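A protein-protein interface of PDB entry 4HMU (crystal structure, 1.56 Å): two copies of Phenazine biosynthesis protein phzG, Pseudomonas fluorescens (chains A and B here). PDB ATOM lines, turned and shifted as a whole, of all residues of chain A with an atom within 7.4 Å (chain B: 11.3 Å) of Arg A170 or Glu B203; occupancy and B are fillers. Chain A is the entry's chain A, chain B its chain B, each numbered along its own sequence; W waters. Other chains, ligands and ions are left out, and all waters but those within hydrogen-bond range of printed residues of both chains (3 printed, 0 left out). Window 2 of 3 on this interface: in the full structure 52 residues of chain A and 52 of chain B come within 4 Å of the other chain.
The guanidinium group (NH1) of Arg A166 is in hydrogen-bond range of the backbone carbonyl oxygen (O) of Gln B202, at 2.9 Å. The guanidinium group of Arg A166 is in salt-bridge range of the side-chain carboxylate of Glu B203 (3.1 Å). NE of Arg A170 is in salt-bridge range of OE2 of Glu B203 (3.1 Å).
Among the printed residues, pairs that only touch across the chains: Ala A145 with Arg B204, Met A149 with Glu B203, Met A149 with Arg B204, Met A149 with Leu B205, Met A165 with Gln B224, Met A165 with Pro B225 and Arg A166 with Leu B205.
Water W1 bridges the side-chain amide oxygen (OE1) of Gln B224 (2.7 Å) and the backbone carbonyl oxygen (O) of Val A152 (2.7 Å). Water W3 lies within hydrogen-bond range of the side-chain carboxylate of Glu B207, the backbone carbonyl oxygen of Leu B205, the guanidinium group of Arg A166 and the backbone NH of Gln B202. Water W2 bridges O of Arg A166 (2.9 Å) and OE1 of Glu B203 (3.3 Å).
Of the printed residues of chain B, Met A165 touches Gln B224 (3.2 Å) and Pro B225 (3.7 Å). No residue of chain B comes within 4 Å of Ala A168. No residue of chain B comes within 4 Å of Ala A169. Arg A170 touches one residue of chain B. No residue of chain B comes within 4 Å of Leu A172. No residue of chain B comes within 4 Å of Ala A173. No residue of chain B comes within 4 Å of Glu A174. Of chain A, only Met A149 (3.5 Å), Arg A166 (3.1 Å) and Arg A170 (3.1 Å) come within 4 Å of Glu B203. Of the printed residues of chain A, Arg B204 touches Ala A145 and Met A149. Of the printed residues of chain A, Gln B224 touches Met A165. The nearest residue of chain A that does not touch Glu B203 is Ala A169 (5.8 Å).
Of the 15 printed residues of chain B, 6 touch a printed residue of chain A. Of the 17 printed residues of chain A, 5 touch a printed residue of chain B. Printed residues of chain A that touch a printed residue of chain B: Ala A145, Met A149, Met A165, Arg A166 and Arg A170. Hydrophobic or aromatic side chains of chain A that line the printed part of chain B: Ala A145, Met A149 and Met A165. Among the printed residues, Asp or Glu carboxylates within 4 Å of a Lys or Arg side-chain nitrogen of the other chain: Arg A166 with Glu B203 and Arg A170 with Glu B203.
No position is printed for both chains.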
ATOM      1  N   ALA A 145       7.125   2.412   1.963  1.00  0.00           N
ATOM      2  CA  ALA A 145       7.872   3.360   1.133  1.00  0.00           C
ATOM      3  C   ALA A 145       8.754   4.295   1.966  1.00  0.00           C
ATOM      4  O   ALA A 145       9.679   4.915   1.430  1.00  0.00           O
ATOM      5  CB  ALA A 145       6.922   4.170   0.269  1.00  0.00           C
ATOM      6  N   PRO A 148      13.109   2.790   3.268  1.00  0.00           N
ATOM      7  CA  PRO A 148      14.457   2.989   2.716  1.00  0.00           C
ATOM      8  C   PRO A 148      15.189   4.216   3.269  1.00  0.00           C
ATOM      9  O   PRO A 148      16.323   4.071   3.733  1.00  0.00           O
ATOM     10  CB  PRO A 148      14.204   3.118   1.203  1.00  0.00           C
ATOM     11  CG  PRO A 148      12.975   2.278   0.980  1.00  0.00           C
ATOM     12  CD  PRO A 148      12.119   2.522   2.208  1.00  0.00           C
ATOM     13  N   MET A 149      14.572   5.397   3.245  1.00  0.00           N
ATOM     14  CA  MET A 149      15.283   6.587   3.705  1.00  0.00           C
ATOM     15  C   MET A 149      15.502   6.534   5.220  1.00  0.00           C
ATOM     16  O   MET A 149      16.554   6.925   5.712  1.00  0.00           O
ATOM     17  CB  MET A 149      14.546   7.865   3.303  1.00  0.00           C
ATOM     18  CG  MET A 149      15.387   9.121   3.470  1.00  0.00           C
ATOM     19  SD  MET A 149      16.863   9.154   2.416  1.00  0.00           S
ATOM     20  CE  MET A 149      16.132   9.097   0.783  1.00  0.00           C
ATOM     21  N   VAL A 152      18.654   4.356   5.871  1.00  0.00           N
ATOM     22  CA  VAL A 152      19.967   4.874   5.492  1.00  0.00           C
ATOM     23  C   VAL A 152      20.355   6.138   6.262  1.00  0.00           C
ATOM     24  O   VAL A 152      21.538   6.411   6.447  1.00  0.00           O
ATOM     25  CB  VAL A 152      20.085   5.134   3.956  1.00  0.00           C
ATOM     26  CG1 VAL A 152      19.862   3.844   3.173  1.00  0.00           C
ATOM     27  CG2 VAL A 152      19.119   6.212   3.497  1.00  0.00           C
ATOM     28  N   GLN A 163      23.811  13.041  -2.849  1.00  0.00           N
ATOM     29  CA  GLN A 163      23.550  12.049  -3.892  1.00  0.00           C
ATOM     30  C   GLN A 163      23.818  10.629  -3.407  1.00  0.00           C
ATOM     31  O   GLN A 163      23.099   9.695  -3.775  1.00  0.00           O
ATOM     32  CB  GLN A 163      24.375  12.325  -5.152  1.00  0.00           C
ATOM     33  CG  GLN A 163      23.948  11.464  -6.333  1.00  0.00           C
ATOM     34  CD  GLN A 163      22.553  11.810  -6.825  1.00  0.00           C
ATOM     35  OE1 GLN A 163      22.170  12.979  -6.860  1.00  0.00           O
ATOM     36  NE2 GLN A 163      21.783  10.792  -7.201  1.00  0.00           N
ATOM     37  N   ALA A 164      24.848  10.456  -2.586  1.00  0.00           N
ATOM     38  CA  ALA A 164      25.167   9.133  -2.056  1.00  0.00           C
ATOM     39  C   ALA A 164      24.010   8.613  -1.203  1.00  0.00           C
ATOM     40  O   ALA A 164      23.647   7.444  -1.282  1.00  0.00           O
ATOM     41  CB  ALA A 164      26.457   9.172  -1.245  1.00  0.00           C
ATOM     42  N   MET A 165      23.424   9.480  -0.387  1.00  0.00           N
ATOM     43  CA  MET A 165      22.286   9.065   0.421  1.00  0.00           C
ATOM     44  C   MET A 165      21.101   8.726  -0.478  1.00  0.00           C
ATOM     45  O   MET A 165      20.419   7.717  -0.279  1.00  0.00           O
ATOM     46  CB  MET A 165      21.888  10.156   1.416  1.00  0.00           C
ATOM     47  CG  MET A 165      20.622   9.810   2.169  1.00  0.00           C
ATOM     48  SD  MET A 165      20.285  10.883   3.564  1.00  0.00           S
ATOM     49  CE  MET A 165      21.530  10.320   4.712  1.00  0.00           C
ATOM     50  N   ARG A 166      20.854   9.573  -1.472  1.00  0.00           N
ATOM     51  CA  ARG A 166      19.754   9.340  -2.393  1.00  0.00           C
ATOM     52  C   ARG A 166      19.918   7.988  -3.083  1.00  0.00           C
ATOM     53  O   ARG A 166      18.970   7.202  -3.180  1.00  0.00           O
ATOM     54  CB  ARG A 166      19.674  10.462  -3.431  1.00  0.00           C
ATOM     55  CG  ARG A 166      18.368  10.474  -4.202  1.00  0.00           C
ATOM     56  CD  ARG A 166      18.254  11.666  -5.150  1.00  0.00           C
ATOM     57  NE  ARG A 166      18.288  12.959  -4.462  1.00  0.00           N
ATOM     58  CZ  ARG A 166      17.316  13.436  -3.686  1.00  0.00           C
ATOM     59  NH1 ARG A 166      16.214  12.727  -3.452  1.00  0.00           N
ATOM     60  NH2 ARG A 166      17.457  14.626  -3.123  1.00  0.00           N
ATOM     61  N   ASN A 167      21.128   7.706  -3.551  1.00  0.00           N
ATOM     62  CA  ASN A 167      21.373   6.465  -4.280  1.00  0.00           C
ATOM     63  C   ASN A 167      21.265   5.225  -3.397  1.00  0.00           C
ATOM     64  O   ASN A 167      20.759   4.195  -3.835  1.00  0.00           O
ATOM     65  CB  ASN A 167      22.738   6.509  -4.973  1.00  0.00           C
ATOM     66  CG  ASN A 167      22.757   7.465  -6.147  1.00  0.00           C
ATOM     67  OD1 ASN A 167      21.725   8.011  -6.530  1.00  0.00           O
ATOM     68  ND2 ASN A 167      23.931   7.664  -6.730  1.00  0.00           N
ATOM     69  N   ALA A 168      21.738   5.326  -2.158  1.00  0.00           N
ATOM     70  CA  ALA A 168      21.659   4.204  -1.233  1.00  0.00           C
ATOM     71  C   ALA A 168      20.198   3.881  -0.924  1.00  0.00           C
ATOM     72  O   ALA A 168      19.801   2.717  -0.909  1.00  0.00           O
ATOM     73  CB  ALA A 168      22.425   4.504   0.044  1.00  0.00           C
ATOM     74  N   ALA A 169      19.392   4.908  -0.666  1.00  0.00           N
ATOM     75  CA  ALA A 169      17.966   4.692  -0.430  1.00  0.00           C
ATOM     76  C   ALA A 169      17.277   4.084  -1.652  1.00  0.00           C
ATOM     77  O   ALA A 169      16.413   3.217  -1.510  1.00  0.00           O
ATOM     78  CB  ALA A 169      17.284   5.989  -0.021  1.00  0.00           C
ATOM     79  N   ARG A 170      17.650   4.536  -2.848  1.00  0.00           N
ATOM     80  CA  ARG A 170      17.066   4.003  -4.080  1.00  0.00           C
ATOM     81  C   ARG A 170      17.309   2.505  -4.206  1.00  0.00           C
ATOM     82  O   ARG A 170      16.443   1.759  -4.670  1.00  0.00           O
ATOM     83  CB  ARG A 170      17.633   4.722  -5.307  1.00  0.00           C
ATOM     84  CG  ARG A 170      17.041   6.100  -5.516  1.00  0.00           C
ATOM     85  CD  ARG A 170      17.673   6.828  -6.681  1.00  0.00           C
ATOM     86  NE  ARG A 170      17.035   8.121  -6.902  1.00  0.00           N
ATOM     87  CZ  ARG A 170      17.377   8.971  -7.865  1.00  0.00           C
ATOM     88  NH1 ARG A 170      18.354   8.668  -8.709  1.00  0.00           N
ATOM     89  NH2 ARG A 170      16.736  10.125  -7.986  1.00  0.00           N
ATOM     90  N   GLN A 171      18.493   2.068  -3.795  1.00  0.00           N
ATOM     91  CA  GLN A 171      18.819   0.650  -3.813  1.00  0.00           C
ATOM     92  C   GLN A 171      17.840  -0.126  -2.938  1.00  0.00           C
ATOM     93  O   GLN A 171      17.368  -1.197  -3.321  1.00  0.00           O
ATOM     94  CB  GLN A 171      20.253   0.427  -3.334  1.00  0.00           C
ATOM     95  CG  GLN A 171      21.304   0.706  -4.390  1.00  0.00           C
ATOM     96  CD  GLN A 171      21.473  -0.453  -5.356  1.00  0.00           C
ATOM     97  OE1 GLN A 171      20.705  -1.412  -5.335  1.00  0.00           O
ATOM     98  NE2 GLN A 171      22.489  -0.371  -6.201  1.00  0.00           N
ATOM     99  N   LEU A 172      17.533   0.415  -1.762  1.00  0.00           N
ATOM    100  CA  LEU A 172      16.621  -0.261  -0.839  1.00  0.00           C
ATOM    101  C   LEU A 172      15.161  -0.160  -1.290  1.00  0.00           C
ATOM    102  O   LEU A 172      14.349  -1.024  -0.959  1.00  0.00           O
ATOM    103  CB  LEU A 172      16.766   0.301   0.589  1.00  0.00           C
ATOM    104  CG  LEU A 172      18.059  -0.022   1.350  1.00  0.00           C
ATOM    105  CD1 LEU A 172      18.035   0.603   2.740  1.00  0.00           C
ATOM    106  CD2 LEU A 172      18.284  -1.535   1.458  1.00  0.00           C
ATOM    107  N   ALA A 173      14.822   0.891  -2.030  1.00  0.00           N
ATOM    108  CA  ALA A 173      13.436   1.108  -2.446  1.00  0.00           C
ATOM    109  C   ALA A 173      12.990   0.073  -3.469  1.00  0.00           C
ATOM    110  O   ALA A 173      11.796  -0.082  -3.726  1.00  0.00           O
ATOM    111  CB  ALA A 173      13.262   2.513  -3.007  1.00  0.00           C
ATOM    112  N   GLU A 174      13.955  -0.633  -4.046  1.00  0.00           N
ATOM    113  CA  GLU A 174      13.660  -1.646  -5.051  1.00  0.00           C
ATOM    114  C   GLU A 174      13.117  -2.913  -4.404  1.00  0.00           C
ATOM    115  O   GLU A 174      12.517  -3.749  -5.073  1.00  0.00           O
ATOM    116  CB  GLU A 174      14.917  -1.979  -5.854  1.00  0.00           C
ATOM    117  CG  GLU A 174      15.381  -0.861  -6.767  1.00  0.00           C
ATOM    118  CD  GLU A 174      16.591  -1.253  -7.588  1.00  0.00           C
ATOM    119  OE1 GLU A 174      17.094  -0.409  -8.357  1.00  0.00           O
ATOM    120  OE2 GLU A 174      17.043  -2.409  -7.462  1.00  0.00           O
ATOM    121  N   LEU A 175      13.335  -3.061  -3.103  1.00  0.00           N
ATOM    122  CA  LEU A 175      12.857  -4.239  -2.391  1.00  0.00           C
ATOM    123  C   LEU A 175      11.364  -4.161  -2.140  1.00  0.00           C
ATOM    124  O   LEU A 175      10.782  -3.078  -2.095  1.00  0.00           O
ATOM    125  CB  LEU A 175      13.568  -4.386  -1.045  1.00  0.00           C
ATOM    126  CG  LEU A 175      14.919  -5.098  -1.075  1.00  0.00           C
ATOM    127  CD1 LEU A 175      15.898  -4.344  -1.950  1.00  0.00           C
ATOM    128  CD2 LEU A 175      15.459  -5.261   0.338  1.00  0.00           C
ATOM    129  N   GLU B  20       1.300   8.589   5.865  1.00  0.00           N
ATOM    130  CA  GLU B  20       2.103   9.790   6.056  1.00  0.00           C
ATOM    131  C   GLU B  20       1.163  10.961   6.310  1.00  0.00           C
ATOM    132  O   GLU B  20       0.094  11.050   5.707  1.00  0.00           O
ATOM    133  CB  GLU B  20       2.970  10.067   4.826  1.00  0.00           C
ATOM    134  N   LEU B  22       1.843  14.364   6.047  1.00  0.00           N
ATOM    135  CA  LEU B  22       2.057  15.609   5.304  1.00  0.00           C
ATOM    136  C   LEU B  22       0.964  15.814   4.270  1.00  0.00           C
ATOM    137  O   LEU B  22       0.630  14.908   3.512  1.00  0.00           O
ATOM    138  CB  LEU B  22       3.412  15.637   4.581  1.00  0.00           C
ATOM    139  CG  LEU B  22       4.701  15.650   5.397  1.00  0.00           C
ATOM    140  CD1 LEU B  22       5.902  15.676   4.455  1.00  0.00           C
ATOM    141  CD2 LEU B  22       4.747  16.830   6.324  1.00  0.00           C
ATOM    142  N   TYR B  33      19.161  25.197  -0.322  1.00  0.00           N
ATOM    143  CA  TYR B  33      19.721  23.909   0.071  1.00  0.00           C
ATOM    144  C   TYR B  33      20.873  23.522  -0.860  1.00  0.00           C
ATOM    145  O   TYR B  33      21.801  22.832  -0.449  1.00  0.00           O
ATOM    146  CB  TYR B  33      18.632  22.844   0.044  1.00  0.00           C
ATOM    147  CG  TYR B  33      19.058  21.466   0.509  1.00  0.00           C
ATOM    148  CD1 TYR B  33      19.266  21.194   1.859  1.00  0.00           C
ATOM    149  CD2 TYR B  33      19.232  20.432  -0.401  1.00  0.00           C
ATOM    150  CE1 TYR B  33      19.629  19.927   2.287  1.00  0.00           C
ATOM    151  CE2 TYR B  33      19.597  19.163   0.019  1.00  0.00           C
ATOM    152  CZ  TYR B  33      19.790  18.914   1.361  1.00  0.00           C
ATOM    153  OH  TYR B  33      20.148  17.645   1.772  1.00  0.00           O
ATOM    154  N   TRP B 198      13.764  23.574   6.880  1.00  0.00           N
ATOM    155  CA  TRP B 198      13.377  22.215   6.541  1.00  0.00           C
ATOM    156  C   TRP B 198      12.362  22.244   5.405  1.00  0.00           C
ATOM    157  O   TRP B 198      11.353  22.946   5.482  1.00  0.00           O
ATOM    158  CB  TRP B 198      12.743  21.559   7.767  1.00  0.00           C
ATOM    159  CG  TRP B 198      12.420  20.074   7.690  1.00  0.00           C
ATOM    160  CD1 TRP B 198      13.121  19.071   8.288  1.00  0.00           C
ATOM    161  CD2 TRP B 198      11.296  19.442   7.039  1.00  0.00           C
ATOM    162  NE1 TRP B 198      12.520  17.865   8.051  1.00  0.00           N
ATOM    163  CE2 TRP B 198      11.409  18.060   7.278  1.00  0.00           C
ATOM    164  CE3 TRP B 198      10.223  19.911   6.276  1.00  0.00           C
ATOM    165  CZ2 TRP B 198      10.481  17.134   6.784  1.00  0.00           C
ATOM    166  CZ3 TRP B 198       9.302  18.989   5.780  1.00  0.00           C
ATOM    167  CH2 TRP B 198       9.440  17.614   6.042  1.00  0.00           C
ATOM    168  N   GLY B 199      12.642  21.481   4.355  1.00  0.00           N
ATOM    169  CA  GLY B 199      11.715  21.292   3.253  1.00  0.00           C
ATOM    170  C   GLY B 199      11.515  19.813   2.981  1.00  0.00           C
ATOM    171  O   GLY B 199      12.350  18.969   3.339  1.00  0.00           O
ATOM    172  N   ASN B 200      10.405  19.486   2.333  1.00  0.00           N
ATOM    173  CA  ASN B 200      10.033  18.098   2.144  1.00  0.00           C
ATOM    174  C   ASN B 200      11.000  17.354   1.218  1.00  0.00           C
ATOM    175  O   ASN B 200      11.205  16.148   1.352  1.00  0.00           O
ATOM    176  CB  ASN B 200       8.607  18.016   1.602  1.00  0.00           C
ATOM    177  CG  ASN B 200       8.075  16.611   1.599  1.00  0.00           C
ATOM    178  OD1 ASN B 200       8.302  15.846   2.542  1.00  0.00           O
ATOM    179  ND2 ASN B 200       7.370  16.250   0.532  1.00  0.00           N
ATOM    180  N   GLY B 201      11.598  18.070   0.276  1.00  0.00           N
ATOM    181  CA  GLY B 201      12.529  17.443  -0.642  1.00  0.00           C
ATOM    182  C   GLY B 201      11.874  16.466  -1.604  1.00  0.00           C
ATOM    183  O   GLY B 201      10.657  16.484  -1.822  1.00  0.00           O
ATOM    184  N   GLN B 202      12.717  15.615  -2.185  1.00  0.00           N
ATOM    185  CA  GLN B 202      12.282  14.593  -3.128  1.00  0.00           C
ATOM    186  C   GLN B 202      12.642  13.213  -2.586  1.00  0.00           C
ATOM    187  O   GLN B 202      13.690  13.039  -1.972  1.00  0.00           O
ATOM    188  CB  GLN B 202      12.960  14.808  -4.484  1.00  0.00           C
ATOM    189  CG  GLN B 202      12.617  16.135  -5.150  1.00  0.00           C
ATOM    190  CD  GLN B 202      13.404  16.376  -6.427  1.00  0.00           C
ATOM    191  OE1 GLN B 202      14.405  15.709  -6.693  1.00  0.00           O
ATOM    192  NE2 GLN B 202      12.949  17.332  -7.228  1.00  0.00           N
ATOM    193  N   GLU B 203      11.763  12.241  -2.817  1.00  0.00           N
ATOM    194  CA  GLU B 203      11.977  10.851  -2.396  1.00  0.00           C
ATOM    195  C   GLU B 203      12.202  10.691  -0.894  1.00  0.00           C
ATOM    196  O   GLU B 203      12.921   9.786  -0.463  1.00  0.00           O
ATOM    197  CB  GLU B 203      13.160  10.242  -3.146  1.00  0.00           C
ATOM    198  CG  GLU B 203      13.027  10.287  -4.656  1.00  0.00           C
ATOM    199  CD  GLU B 203      14.262   9.752  -5.354  1.00  0.00           C
ATOM    200  OE1 GLU B 203      15.363  10.298  -5.127  1.00  0.00           O
ATOM    201  OE2 GLU B 203      14.138   8.782  -6.125  1.00  0.00           O
ATOM    202  N   ARG B 204      11.559  11.555  -0.115  1.00  0.00           N
ATOM    203  CA  ARG B 204      11.655  11.548   1.347  1.00  0.00           C
ATOM    204  C   ARG B 204      13.046  11.924   1.873  1.00  0.00           C
ATOM    205  O   ARG B 204      13.312  11.844   3.080  1.00  0.00           O
ATOM    206  CB  ARG B 204      11.179  10.206   1.911  1.00  0.00           C
ATOM    207  CG  ARG B 204       9.711   9.935   1.579  1.00  0.00           C
ATOM    208  CD  ARG B 204       9.226   8.579   2.042  1.00  0.00           C
ATOM    209  NE  ARG B 204       7.787   8.433   1.801  1.00  0.00           N
ATOM    210  CZ  ARG B 204       7.244   8.019   0.658  1.00  0.00           C
ATOM    211  NH1 ARG B 204       8.006   7.688  -0.378  1.00  0.00           N
ATOM    212  NH2 ARG B 204       5.925   7.933   0.551  1.00  0.00           N
ATOM    213  N   LEU B 205      13.928  12.371   0.983  1.00  0.00           N
ATOM    214  CA  LEU B 205      15.190  12.936   1.444  1.00  0.00           C
ATOM    215  C   LEU B 205      14.890  14.373   1.840  1.00  0.00           C
ATOM    216  O   LEU B 205      15.105  15.317   1.068  1.00  0.00           O
ATOM    217  CB  LEU B 205      16.265  12.878   0.365  1.00  0.00           C
ATOM    218  CG  LEU B 205      17.689  12.833   0.921  1.00  0.00           C
ATOM    219  CD1 LEU B 205      18.684  12.461  -0.167  1.00  0.00           C
ATOM    220  CD2 LEU B 205      18.077  14.156   1.572  1.00  0.00           C
ATOM    221  N   HIS B 206      14.350  14.543   3.036  1.00  0.00           N
ATOM    222  CA  HIS B 206      13.959  15.872   3.465  1.00  0.00           C
ATOM    223  C   HIS B 206      15.185  16.756   3.525  1.00  0.00           C
ATOM    224  O   HIS B 206      16.263  16.314   3.901  1.00  0.00           O
ATOM    225  CB  HIS B 206      13.256  15.823   4.809  1.00  0.00           C
ATOM    226  CG  HIS B 206      12.137  14.830   4.852  1.00  0.00           C
ATOM    227  ND1 HIS B 206      11.124  14.813   3.920  1.00  0.00           N
ATOM    228  CD2 HIS B 206      11.873  13.826   5.720  1.00  0.00           C
ATOM    229  CE1 HIS B 206      10.280  13.836   4.210  1.00  0.00           C
ATOM    230  NE2 HIS B 206      10.714  13.217   5.292  1.00  0.00           N
ATOM    231  N   GLU B 207      14.998  18.006   3.132  1.00  0.00           N
ATOM    232  CA  GLU B 207      16.099  18.937   2.953  1.00  0.00           C
ATOM    233  C   GLU B 207      16.227  19.816   4.184  1.00  0.00           C
ATOM    234  O   GLU B 207      15.332  20.579   4.507  1.00  0.00           O
ATOM    235  CB  GLU B 207      15.891  19.740   1.654  1.00  0.00           C
ATOM    236  CG  GLU B 207      15.968  18.813   0.437  1.00  0.00           C
ATOM    237  CD  GLU B 207      15.636  19.451  -0.894  1.00  0.00           C
ATOM    238  OE1 GLU B 207      15.167  20.613  -0.923  1.00  0.00           O
ATOM    239  OE2 GLU B 207      15.839  18.765  -1.933  1.00  0.00           O
ATOM    240  N   GLN B 224      21.097  15.139   7.949  1.00  0.00           N
ATOM    241  CA  GLN B 224      20.378  13.953   7.504  1.00  0.00           C
ATOM    242  C   GLN B 224      18.939  13.973   8.024  1.00  0.00           C
ATOM    243  O   GLN B 224      18.694  14.342   9.179  1.00  0.00           O
ATOM    244  CB  GLN B 224      21.112  12.692   7.964  1.00  0.00           C
ATOM    245  CG  GLN B 224      22.533  12.623   7.423  1.00  0.00           C
ATOM    246  CD  GLN B 224      23.254  11.323   7.748  1.00  0.00           C
ATOM    247  OE1 GLN B 224      22.677  10.239   7.678  1.00  0.00           O
ATOM    248  NE2 GLN B 224      24.528  11.431   8.104  1.00  0.00           N
ATOM    249  N   PRO B 225      17.986  13.571   7.168  1.00  0.00           N
ATOM    250  CA  PRO B 225      16.556  13.674   7.477  1.00  0.00           C
ATOM    251  C   PRO B 225      16.085  12.732   8.572  1.00  0.00           C
ATOM    252  O   PRO B 225      15.107  13.055   9.254  1.00  0.00           O
ATOM    253  CB  PRO B 225      15.875  13.322   6.150  1.00  0.00           C
ATOM    254  CG  PRO B 225      16.873  12.534   5.393  1.00  0.00           C
ATOM    255  CD  PRO B 225      18.225  13.051   5.811  1.00  0.00           C
ATOM    256  OXT PRO B 225      16.647  11.653   8.794  1.00  0.00           O
HETATM  257  O   HOH W   1      23.633   8.082   6.438  1.00  0.00           O
HETATM  258  O   HOH W   2      16.215   7.963  -2.954  1.00  0.00           O
HETATM  259  O   HOH W   3      15.533  16.038  -1.576  1.00  0.00           O
